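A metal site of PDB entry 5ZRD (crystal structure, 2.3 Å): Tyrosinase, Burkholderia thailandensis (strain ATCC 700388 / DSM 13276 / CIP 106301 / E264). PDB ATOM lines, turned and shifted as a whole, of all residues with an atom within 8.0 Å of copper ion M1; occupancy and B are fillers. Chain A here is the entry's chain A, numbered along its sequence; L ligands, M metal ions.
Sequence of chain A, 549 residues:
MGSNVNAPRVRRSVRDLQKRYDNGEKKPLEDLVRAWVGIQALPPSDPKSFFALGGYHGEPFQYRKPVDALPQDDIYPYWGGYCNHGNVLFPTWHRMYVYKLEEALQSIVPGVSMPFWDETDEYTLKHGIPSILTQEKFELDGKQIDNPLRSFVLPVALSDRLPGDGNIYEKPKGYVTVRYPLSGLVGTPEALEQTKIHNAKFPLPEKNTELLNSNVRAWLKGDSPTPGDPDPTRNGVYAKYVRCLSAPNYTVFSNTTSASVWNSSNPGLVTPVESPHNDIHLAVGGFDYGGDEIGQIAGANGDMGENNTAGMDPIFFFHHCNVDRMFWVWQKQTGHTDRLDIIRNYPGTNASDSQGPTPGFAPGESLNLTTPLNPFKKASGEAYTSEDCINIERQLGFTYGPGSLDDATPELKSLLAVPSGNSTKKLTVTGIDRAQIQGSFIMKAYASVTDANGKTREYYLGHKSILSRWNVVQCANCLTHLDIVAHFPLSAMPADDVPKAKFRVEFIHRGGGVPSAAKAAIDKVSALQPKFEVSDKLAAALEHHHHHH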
ATOM      1  N   HIS A  57      -3.371  20.446 -11.245  1.00  0.00           N
ATOM      2  CA  HIS A  57      -4.333  19.839 -10.362  1.00  0.00           C
ATOM      3  C   HIS A  57      -5.059  18.694 -11.075  1.00  0.00           C
ATOM      4  O   HIS A  57      -5.049  17.547 -10.617  1.00  0.00           O
ATOM      5  CB  HIS A  57      -5.345  20.894  -9.891  1.00  0.00           C
ATOM      6  CG  HIS A  57      -6.185  20.422  -8.767  1.00  0.00           C
ATOM      7  ND1 HIS A  57      -7.477  20.005  -8.944  1.00  0.00           N
ATOM      8  CD2 HIS A  57      -5.889  20.226  -7.456  1.00  0.00           C
ATOM      9  CE1 HIS A  57      -7.962  19.619  -7.786  1.00  0.00           C
ATOM     10  NE2 HIS A  57      -6.994  19.716  -6.865  1.00  0.00           N
ATOM     11  N   CYS A  83      -3.155  15.905  -8.717  1.00  0.00           N
ATOM     12  CA  CYS A  83      -3.592  16.114  -7.352  1.00  0.00           C
ATOM     13  C   CYS A  83      -3.933  14.748  -6.755  1.00  0.00           C
ATOM     14  O   CYS A  83      -4.389  13.817  -7.483  1.00  0.00           O
ATOM     15  CB  CYS A  83      -4.720  17.123  -7.240  1.00  0.00           C
ATOM     16  SG  CYS A  83      -6.325  16.540  -7.885  1.00  0.00           S
ATOM     17  N   ASN A  84      -3.639  14.627  -5.451  1.00  0.00           N
ATOM     18  CA  ASN A  84      -3.962  13.458  -4.627  1.00  0.00           C
ATOM     19  C   ASN A  84      -5.264  13.738  -3.846  1.00  0.00           C
ATOM     20  O   ASN A  84      -5.341  14.722  -3.098  1.00  0.00           O
ATOM     21  CB  ASN A  84      -2.828  13.113  -3.665  1.00  0.00           C
ATOM     22  CG  ASN A  84      -1.733  12.318  -4.321  1.00  0.00           C
ATOM     23  OD1 ASN A  84      -1.934  11.135  -4.573  1.00  0.00           O
ATOM     24  ND2 ASN A  84      -0.619  12.955  -4.650  1.00  0.00           N
ATOM     25  N   HIS A  85      -6.230  12.815  -3.984  1.00  0.00           N
ATOM     26  CA  HIS A  85      -7.544  12.868  -3.316  1.00  0.00           C
ATOM     27  C   HIS A  85      -7.968  11.475  -2.845  1.00  0.00           C
ATOM     28  O   HIS A  85      -7.627  10.489  -3.450  1.00  0.00           O
ATOM     29  CB  HIS A  85      -8.604  13.399  -4.277  1.00  0.00           C
ATOM     30  CG  HIS A  85      -8.193  14.694  -4.882  1.00  0.00           C
ATOM     31  ND1 HIS A  85      -7.525  14.768  -6.060  1.00  0.00           N
ATOM     32  CD2 HIS A  85      -8.256  15.961  -4.398  1.00  0.00           C
ATOM     33  CE1 HIS A  85      -7.255  16.029  -6.311  1.00  0.00           C
ATOM     34  NE2 HIS A  85      -7.689  16.790  -5.314  1.00  0.00           N
ATOM     35  N   PHE A  90      -3.240  13.517   0.425  1.00  0.00           N
ATOM     36  CA  PHE A  90      -4.080  14.706   0.164  1.00  0.00           C
ATOM     37  C   PHE A  90      -3.474  15.972   0.837  1.00  0.00           C
ATOM     38  O   PHE A  90      -3.325  17.004   0.201  1.00  0.00           O
ATOM     39  CB  PHE A  90      -5.541  14.437   0.544  1.00  0.00           C
ATOM     40  CG  PHE A  90      -6.355  15.698   0.672  1.00  0.00           C
ATOM     41  CD1 PHE A  90      -6.962  16.268  -0.424  1.00  0.00           C
ATOM     42  CD2 PHE A  90      -6.438  16.371   1.878  1.00  0.00           C
ATOM     43  CE1 PHE A  90      -7.674  17.455  -0.312  1.00  0.00           C
ATOM     44  CE2 PHE A  90      -7.158  17.541   2.002  1.00  0.00           C
ATOM     45  CZ  PHE A  90      -7.784  18.085   0.896  1.00  0.00           C
ATOM     46  N   TRP A  93       0.298  16.887  -0.444  1.00  0.00           N
ATOM     47  CA  TRP A  93       0.369  17.244  -1.857  1.00  0.00           C
ATOM     48  C   TRP A  93      -0.135  18.658  -2.007  1.00  0.00           C
ATOM     49  O   TRP A  93       0.511  19.443  -2.721  1.00  0.00           O
ATOM     50  CB  TRP A  93      -0.399  16.290  -2.761  1.00  0.00           C
ATOM     51  CG  TRP A  93      -0.186  16.610  -4.209  1.00  0.00           C
ATOM     52  CD1 TRP A  93       0.819  16.125  -4.999  1.00  0.00           C
ATOM     53  CD2 TRP A  93      -0.935  17.542  -5.005  1.00  0.00           C
ATOM     54  NE1 TRP A  93       0.717  16.667  -6.251  1.00  0.00           N
ATOM     55  CE2 TRP A  93      -0.331  17.562  -6.284  1.00  0.00           C
ATOM     56  CE3 TRP A  93      -2.043  18.365  -4.775  1.00  0.00           C
ATOM     57  CZ2 TRP A  93      -0.792  18.356  -7.315  1.00  0.00           C
ATOM     58  CZ3 TRP A  93      -2.495  19.156  -5.796  1.00  0.00           C
ATOM     59  CH2 TRP A  93      -1.886  19.143  -7.052  1.00  0.00           C
ATOM     60  N   HIS A  94      -1.290  18.957  -1.396  1.00  0.00           N
ATOM     61  CA  HIS A  94      -1.859  20.290  -1.545  1.00  0.00           C
ATOM     62  C   HIS A  94      -0.978  21.308  -0.827  1.00  0.00           C
ATOM     63  O   HIS A  94      -0.938  22.426  -1.258  1.00  0.00           O
ATOM     64  CB  HIS A  94      -3.304  20.386  -1.083  1.00  0.00           C
ATOM     65  CG  HIS A  94      -4.204  19.668  -2.008  1.00  0.00           C
ATOM     66  ND1 HIS A  94      -4.296  18.326  -1.975  1.00  0.00           N
ATOM     67  CD2 HIS A  94      -4.988  20.086  -3.026  1.00  0.00           C
ATOM     68  CE1 HIS A  94      -5.108  17.926  -2.939  1.00  0.00           C
ATOM     69  NE2 HIS A  94      -5.570  18.998  -3.581  1.00  0.00           N
ATOM     70  N   TYR A  97       1.421  22.155  -3.339  1.00  0.00           N
ATOM     71  CA  TYR A  97       0.771  22.826  -4.467  1.00  0.00           C
ATOM     72  C   TYR A  97       0.652  24.313  -4.157  1.00  0.00           C
ATOM     73  O   TYR A  97       0.988  25.152  -5.003  1.00  0.00           O
ATOM     74  CB  TYR A  97      -0.602  22.220  -4.768  1.00  0.00           C
ATOM     75  CG  TYR A  97      -1.296  22.654  -6.041  1.00  0.00           C
ATOM     76  CD1 TYR A  97      -0.618  23.193  -7.125  1.00  0.00           C
ATOM     77  CD2 TYR A  97      -2.661  22.474  -6.175  1.00  0.00           C
ATOM     78  CE1 TYR A  97      -1.271  23.539  -8.308  1.00  0.00           C
ATOM     79  CE2 TYR A  97      -3.314  22.766  -7.353  1.00  0.00           C
ATOM     80  CZ  TYR A  97      -2.625  23.312  -8.416  1.00  0.00           C
ATOM     81  OH  TYR A  97      -3.293  23.635  -9.547  1.00  0.00           O
ATOM     82  N   GLU A 274     -10.174  16.456   4.731  1.00  0.00           N
ATOM     83  CA  GLU A 274     -10.634  16.381   3.348  1.00  0.00           C
ATOM     84  C   GLU A 274     -12.153  16.608   3.229  1.00  0.00           C
ATOM     85  O   GLU A 274     -12.619  17.026   2.167  1.00  0.00           O
ATOM     86  CB  GLU A 274     -10.277  15.042   2.704  1.00  0.00           C
ATOM     87  CG  GLU A 274     -10.297  15.086   1.198  1.00  0.00           C
ATOM     88  CD  GLU A 274      -9.908  13.805   0.481  1.00  0.00           C
ATOM     89  OE1 GLU A 274      -9.790  13.826  -0.799  1.00  0.00           O
ATOM     90  OE2 GLU A 274      -9.791  12.756   1.192  1.00  0.00           O
ATOM     91  N   HIS A 277     -13.328  20.288   3.529  1.00  0.00           N
ATOM     92  CA  HIS A 277     -12.693  20.750   2.277  1.00  0.00           C
ATOM     93  C   HIS A 277     -13.620  20.483   1.081  1.00  0.00           C
ATOM     94  O   HIS A 277     -13.929  21.391   0.335  1.00  0.00           O
ATOM     95  CB  HIS A 277     -11.313  20.132   2.084  1.00  0.00           C
ATOM     96  CG  HIS A 277     -10.933  19.901   0.666  1.00  0.00           C
ATOM     97  ND1 HIS A 277     -11.324  18.762  -0.029  1.00  0.00           N
ATOM     98  CD2 HIS A 277     -10.180  20.614  -0.194  1.00  0.00           C
ATOM     99  CE1 HIS A 277     -10.829  18.796  -1.258  1.00  0.00           C
ATOM    100  NE2 HIS A 277     -10.114  19.905  -1.389  1.00  0.00           N
ATOM    101  N   ASN A 278     -14.012  19.231   0.929  1.00  0.00           N
ATOM    102  CA  ASN A 278     -14.987  18.820  -0.068  1.00  0.00           C
ATOM    103  C   ASN A 278     -16.214  19.746  -0.039  1.00  0.00           C
ATOM    104  O   ASN A 278     -16.658  20.219  -1.103  1.00  0.00           O
ATOM    105  CB  ASN A 278     -15.371  17.353   0.100  1.00  0.00           C
ATOM    106  CG  ASN A 278     -14.289  16.401  -0.342  1.00  0.00           C
ATOM    107  OD1 ASN A 278     -13.209  16.821  -0.747  1.00  0.00           O
ATOM    108  ND2 ASN A 278     -14.565  15.103  -0.259  1.00  0.00           N
ATOM    109  N   ILE A 280     -16.584  22.858   0.791  1.00  0.00           N
ATOM    110  CA  ILE A 280     -16.363  24.216   0.366  1.00  0.00           C
ATOM    111  C   ILE A 280     -16.295  24.202  -1.158  1.00  0.00           C
ATOM    112  O   ILE A 280     -16.816  25.072  -1.798  1.00  0.00           O
ATOM    113  CB  ILE A 280     -15.102  24.842   1.037  1.00  0.00           C
ATOM    114  CG1 ILE A 280     -15.285  25.127   2.529  1.00  0.00           C
ATOM    115  CG2 ILE A 280     -14.651  26.094   0.328  1.00  0.00           C
ATOM    116  CD1 ILE A 280     -16.454  26.056   2.895  1.00  0.00           C
ATOM    117  N   HIS A 281     -15.616  23.234  -1.725  1.00  0.00           N
ATOM    118  CA  HIS A 281     -15.641  23.046  -3.141  1.00  0.00           C
ATOM    119  C   HIS A 281     -17.091  22.947  -3.651  1.00  0.00           C
ATOM    120  O   HIS A 281     -17.386  23.513  -4.660  1.00  0.00           O
ATOM    121  CB  HIS A 281     -14.896  21.759  -3.505  1.00  0.00           C
ATOM    122  CG  HIS A 281     -13.428  21.916  -3.673  1.00  0.00           C
ATOM    123  ND1 HIS A 281     -12.847  22.054  -4.914  1.00  0.00           N
ATOM    124  CD2 HIS A 281     -12.415  21.875  -2.777  1.00  0.00           C
ATOM    125  CE1 HIS A 281     -11.532  22.083  -4.772  1.00  0.00           C
ATOM    126  NE2 HIS A 281     -11.245  22.030  -3.454  1.00  0.00           N
ATOM    127  N   MET A 304     -15.041  24.918  -9.508  1.00  0.00           N
ATOM    128  CA  MET A 304     -14.644  24.433  -8.175  1.00  0.00           C
ATOM    129  C   MET A 304     -15.406  23.151  -7.773  1.00  0.00           C
ATOM    130  O   MET A 304     -15.002  22.484  -6.837  1.00  0.00           O
ATOM    131  CB  MET A 304     -14.904  25.516  -7.118  1.00  0.00           C
ATOM    132  CG  MET A 304     -13.773  26.525  -6.983  1.00  0.00           C
ATOM    133  SD  MET A 304     -12.273  25.839  -6.233  1.00  0.00           S
ATOM    134  CE  MET A 304     -12.818  25.566  -4.556  1.00  0.00           C
ATOM    135  N   GLU A 306     -15.859  20.163  -9.096  1.00  0.00           N
ATOM    136  CA  GLU A 306     -15.277  18.897  -9.475  1.00  0.00           C
ATOM    137  C   GLU A 306     -13.750  19.108  -9.603  1.00  0.00           C
ATOM    138  O   GLU A 306     -13.254  20.254  -9.675  1.00  0.00           O
ATOM    139  CB  GLU A 306     -15.812  18.401 -10.820  1.00  0.00           C
ATOM    140  CG  GLU A 306     -17.167  17.675 -10.756  1.00  0.00           C
ATOM    141  CD  GLU A 306     -18.429  18.497 -10.510  1.00  0.00           C
ATOM    142  OE1 GLU A 306     -18.411  19.723 -10.670  1.00  0.00           O
ATOM    143  OE2 GLU A 306     -19.453  17.879 -10.144  1.00  0.00           O
ATOM    144  N   ASN A 307     -12.984  18.034  -9.609  1.00  0.00           N
ATOM    145  CA  ASN A 307     -11.558  18.187  -9.529  1.00  0.00           C
ATOM    146  C   ASN A 307     -11.007  18.590 -10.915  1.00  0.00           C
ATOM    147  O   ASN A 307      -9.863  19.042 -11.014  1.00  0.00           O
ATOM    148  CB  ASN A 307     -10.921  16.933  -8.968  1.00  0.00           C
ATOM    149  CG  ASN A 307     -10.998  16.863  -7.458  1.00  0.00           C
ATOM    150  OD1 ASN A 307     -11.160  15.780  -6.889  1.00  0.00           O
ATOM    151  ND2 ASN A 307     -10.895  18.008  -6.788  1.00  0.00           N
ATOM    152  N   ALA A 310     -11.136  22.784 -11.141  1.00  0.00           N
ATOM    153  CA  ALA A 310     -11.176  23.646  -9.936  1.00  0.00           C
ATOM    154  C   ALA A 310      -9.890  24.452  -9.781  1.00  0.00           C
ATOM    155  O   ALA A 310      -9.892  25.556  -9.268  1.00  0.00           O
ATOM    156  CB  ALA A 310     -11.358  22.784  -8.723  1.00  0.00           C
ATOM    157  N   GLY A 311      -8.764  23.873 -10.170  1.00  0.00           N
ATOM    158  CA  GLY A 311      -7.474  24.582 -10.006  1.00  0.00           C
ATOM    159  C   GLY A 311      -7.381  25.841 -10.867  1.00  0.00           C
ATOM    160  O   GLY A 311      -6.484  26.646 -10.635  1.00  0.00           O
ATOM    161  N   PHE A 316      -9.511  28.645  -5.542  1.00  0.00           N
ATOM    162  CA  PHE A 316      -8.924  27.349  -5.153  1.00  0.00           C
ATOM    163  C   PHE A 316      -7.757  27.531  -4.171  1.00  0.00           C
ATOM    164  O   PHE A 316      -7.677  26.822  -3.199  1.00  0.00           O
ATOM    165  CB  PHE A 316      -8.436  26.577  -6.366  1.00  0.00           C
ATOM    166  CG  PHE A 316      -7.827  25.237  -6.032  1.00  0.00           C
ATOM    167  CD1 PHE A 316      -6.503  25.144  -5.648  1.00  0.00           C
ATOM    168  CD2 PHE A 316      -8.578  24.078  -6.132  1.00  0.00           C
ATOM    169  CE1 PHE A 316      -5.954  23.912  -5.359  1.00  0.00           C
ATOM    170  CE2 PHE A 316      -8.035  22.838  -5.822  1.00  0.00           C
ATOM    171  CZ  PHE A 316      -6.726  22.762  -5.431  1.00  0.00           C
ATOM    172  N   PHE A 317      -6.901  28.503  -4.389  1.00  0.00           N
ATOM    173  CA  PHE A 317      -5.634  28.590  -3.652  1.00  0.00           C
ATOM    174  C   PHE A 317      -5.847  29.280  -2.297  1.00  0.00           C
ATOM    175  O   PHE A 317      -5.169  28.936  -1.314  1.00  0.00           O
ATOM    176  CB  PHE A 317      -4.568  29.242  -4.530  1.00  0.00           C
ATOM    177  CG  PHE A 317      -4.197  28.317  -5.640  1.00  0.00           C
ATOM    178  CD1 PHE A 317      -4.953  28.275  -6.790  1.00  0.00           C
ATOM    179  CD2 PHE A 317      -3.240  27.348  -5.448  1.00  0.00           C
ATOM    180  CE1 PHE A 317      -4.686  27.343  -7.778  1.00  0.00           C
ATOM    181  CE2 PHE A 317      -2.959  26.421  -6.445  1.00  0.00           C
ATOM    182  CZ  PHE A 317      -3.686  26.421  -7.605  1.00  0.00           C
ATOM    183  N   HIS A 319      -8.601  28.991  -0.577  1.00  0.00           N
ATOM    184  CA  HIS A 319      -9.276  27.937   0.126  1.00  0.00           C
ATOM    185  C   HIS A 319      -8.265  26.896   0.632  1.00  0.00           C
ATOM    186  O   HIS A 319      -8.297  26.512   1.799  1.00  0.00           O
ATOM    187  CB  HIS A 319     -10.287  27.263  -0.802  1.00  0.00           C
ATOM    188  CG  HIS A 319     -10.704  25.909  -0.353  1.00  0.00           C
ATOM    189  ND1 HIS A 319     -11.372  25.695   0.825  1.00  0.00           N
ATOM    190  CD2 HIS A 319     -10.540  24.705  -0.925  1.00  0.00           C
ATOM    191  CE1 HIS A 319     -11.656  24.412   0.937  1.00  0.00           C
ATOM    192  NE2 HIS A 319     -11.112  23.776  -0.112  1.00  0.00           N
ATOM    193  N   HIS A 320      -7.436  26.423  -0.275  1.00  0.00           N
ATOM    194  CA  HIS A 320      -6.460  25.431   0.042  1.00  0.00           C
ATOM    195  C   HIS A 320      -5.372  25.965   0.958  1.00  0.00           C
ATOM    196  O   HIS A 320      -4.757  25.157   1.641  1.00  0.00           O
ATOM    197  CB  HIS A 320      -5.859  24.795  -1.213  1.00  0.00           C
ATOM    198  CG  HIS A 320      -6.551  23.525  -1.541  1.00  0.00           C
ATOM    199  ND1 HIS A 320      -6.280  22.358  -0.878  1.00  0.00           N
ATOM    200  CD2 HIS A 320      -7.543  23.246  -2.409  1.00  0.00           C
ATOM    201  CE1 HIS A 320      -7.067  21.412  -1.331  1.00  0.00           C
ATOM    202  NE2 HIS A 320      -7.824  21.919  -2.284  1.00  0.00           N
ATOM    203  N   VAL A 323      -7.050  25.227   4.147  1.00  0.00           N
ATOM    204  CA  VAL A 323      -7.036  23.823   4.445  1.00  0.00           C
ATOM    205  C   VAL A 323      -5.643  23.462   4.998  1.00  0.00           C
ATOM    206  O   VAL A 323      -5.487  22.588   5.869  1.00  0.00           O
ATOM    207  CB  VAL A 323      -7.379  23.016   3.183  1.00  0.00           C
ATOM    208  CG1 VAL A 323      -7.192  21.525   3.372  1.00  0.00           C
ATOM    209  CG2 VAL A 323      -8.808  23.300   2.764  1.00  0.00           C
ATOM    210  N   LEU A 467     -16.648  14.950  -3.367  1.00  0.00           N
ATOM    211  CA  LEU A 467     -16.001  15.718  -4.422  1.00  0.00           C
ATOM    212  C   LEU A 467     -15.431  14.730  -5.409  1.00  0.00           C
ATOM    213  O   LEU A 467     -14.594  13.926  -5.029  1.00  0.00           O
ATOM    214  CB  LEU A 467     -14.868  16.543  -3.828  1.00  0.00           C
ATOM    215  CG  LEU A 467     -14.045  17.374  -4.802  1.00  0.00           C
ATOM    216  CD1 LEU A 467     -14.914  18.413  -5.497  1.00  0.00           C
ATOM    217  CD2 LEU A 467     -12.898  18.060  -4.055  1.00  0.00           C
HETATM  218  O1  LIG L   1      -9.201  19.476  -4.034  1.00  0.00           O
HETATM  219 CU    CU M   1      -9.474  21.292  -2.878  1.00  0.00          CU
HETATM  220 CU    CU M   2      -7.082  18.768  -5.102  1.00  0.00          CU
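A ring nitrogen (ND1) of His 277 lies within hydrogen-bond range of the side-chain amide oxygen (OD1) of Asn 278 (2.8 Å). ND1 of His 277 sits at hydrogen-bond distance from O of Glu 274, at 3.1 Å. ND1 of His 281 is in hydrogen-bond range of O of Met 304.
CE2 of Phe 316 touches copper ion M1, 3.6 Å away. Of the 24 residues printed, 4 come within 4 Å of copper ion M1. The nearest printed residue that does not touch copper ion M1 is His 319 (4.1 Å).
Copper ion M1 is bound by a ring nitrogen (NE2) of His 320 (1.9 Å), a ring nitrogen (NE2) of His 281 (2.0 Å), a ring nitrogen (NE2) of His 277 (2.1 Å) and an oxygen (O1) of the ligand (2.2 Å). Copper ion M1 has four donor atoms within binding distance.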
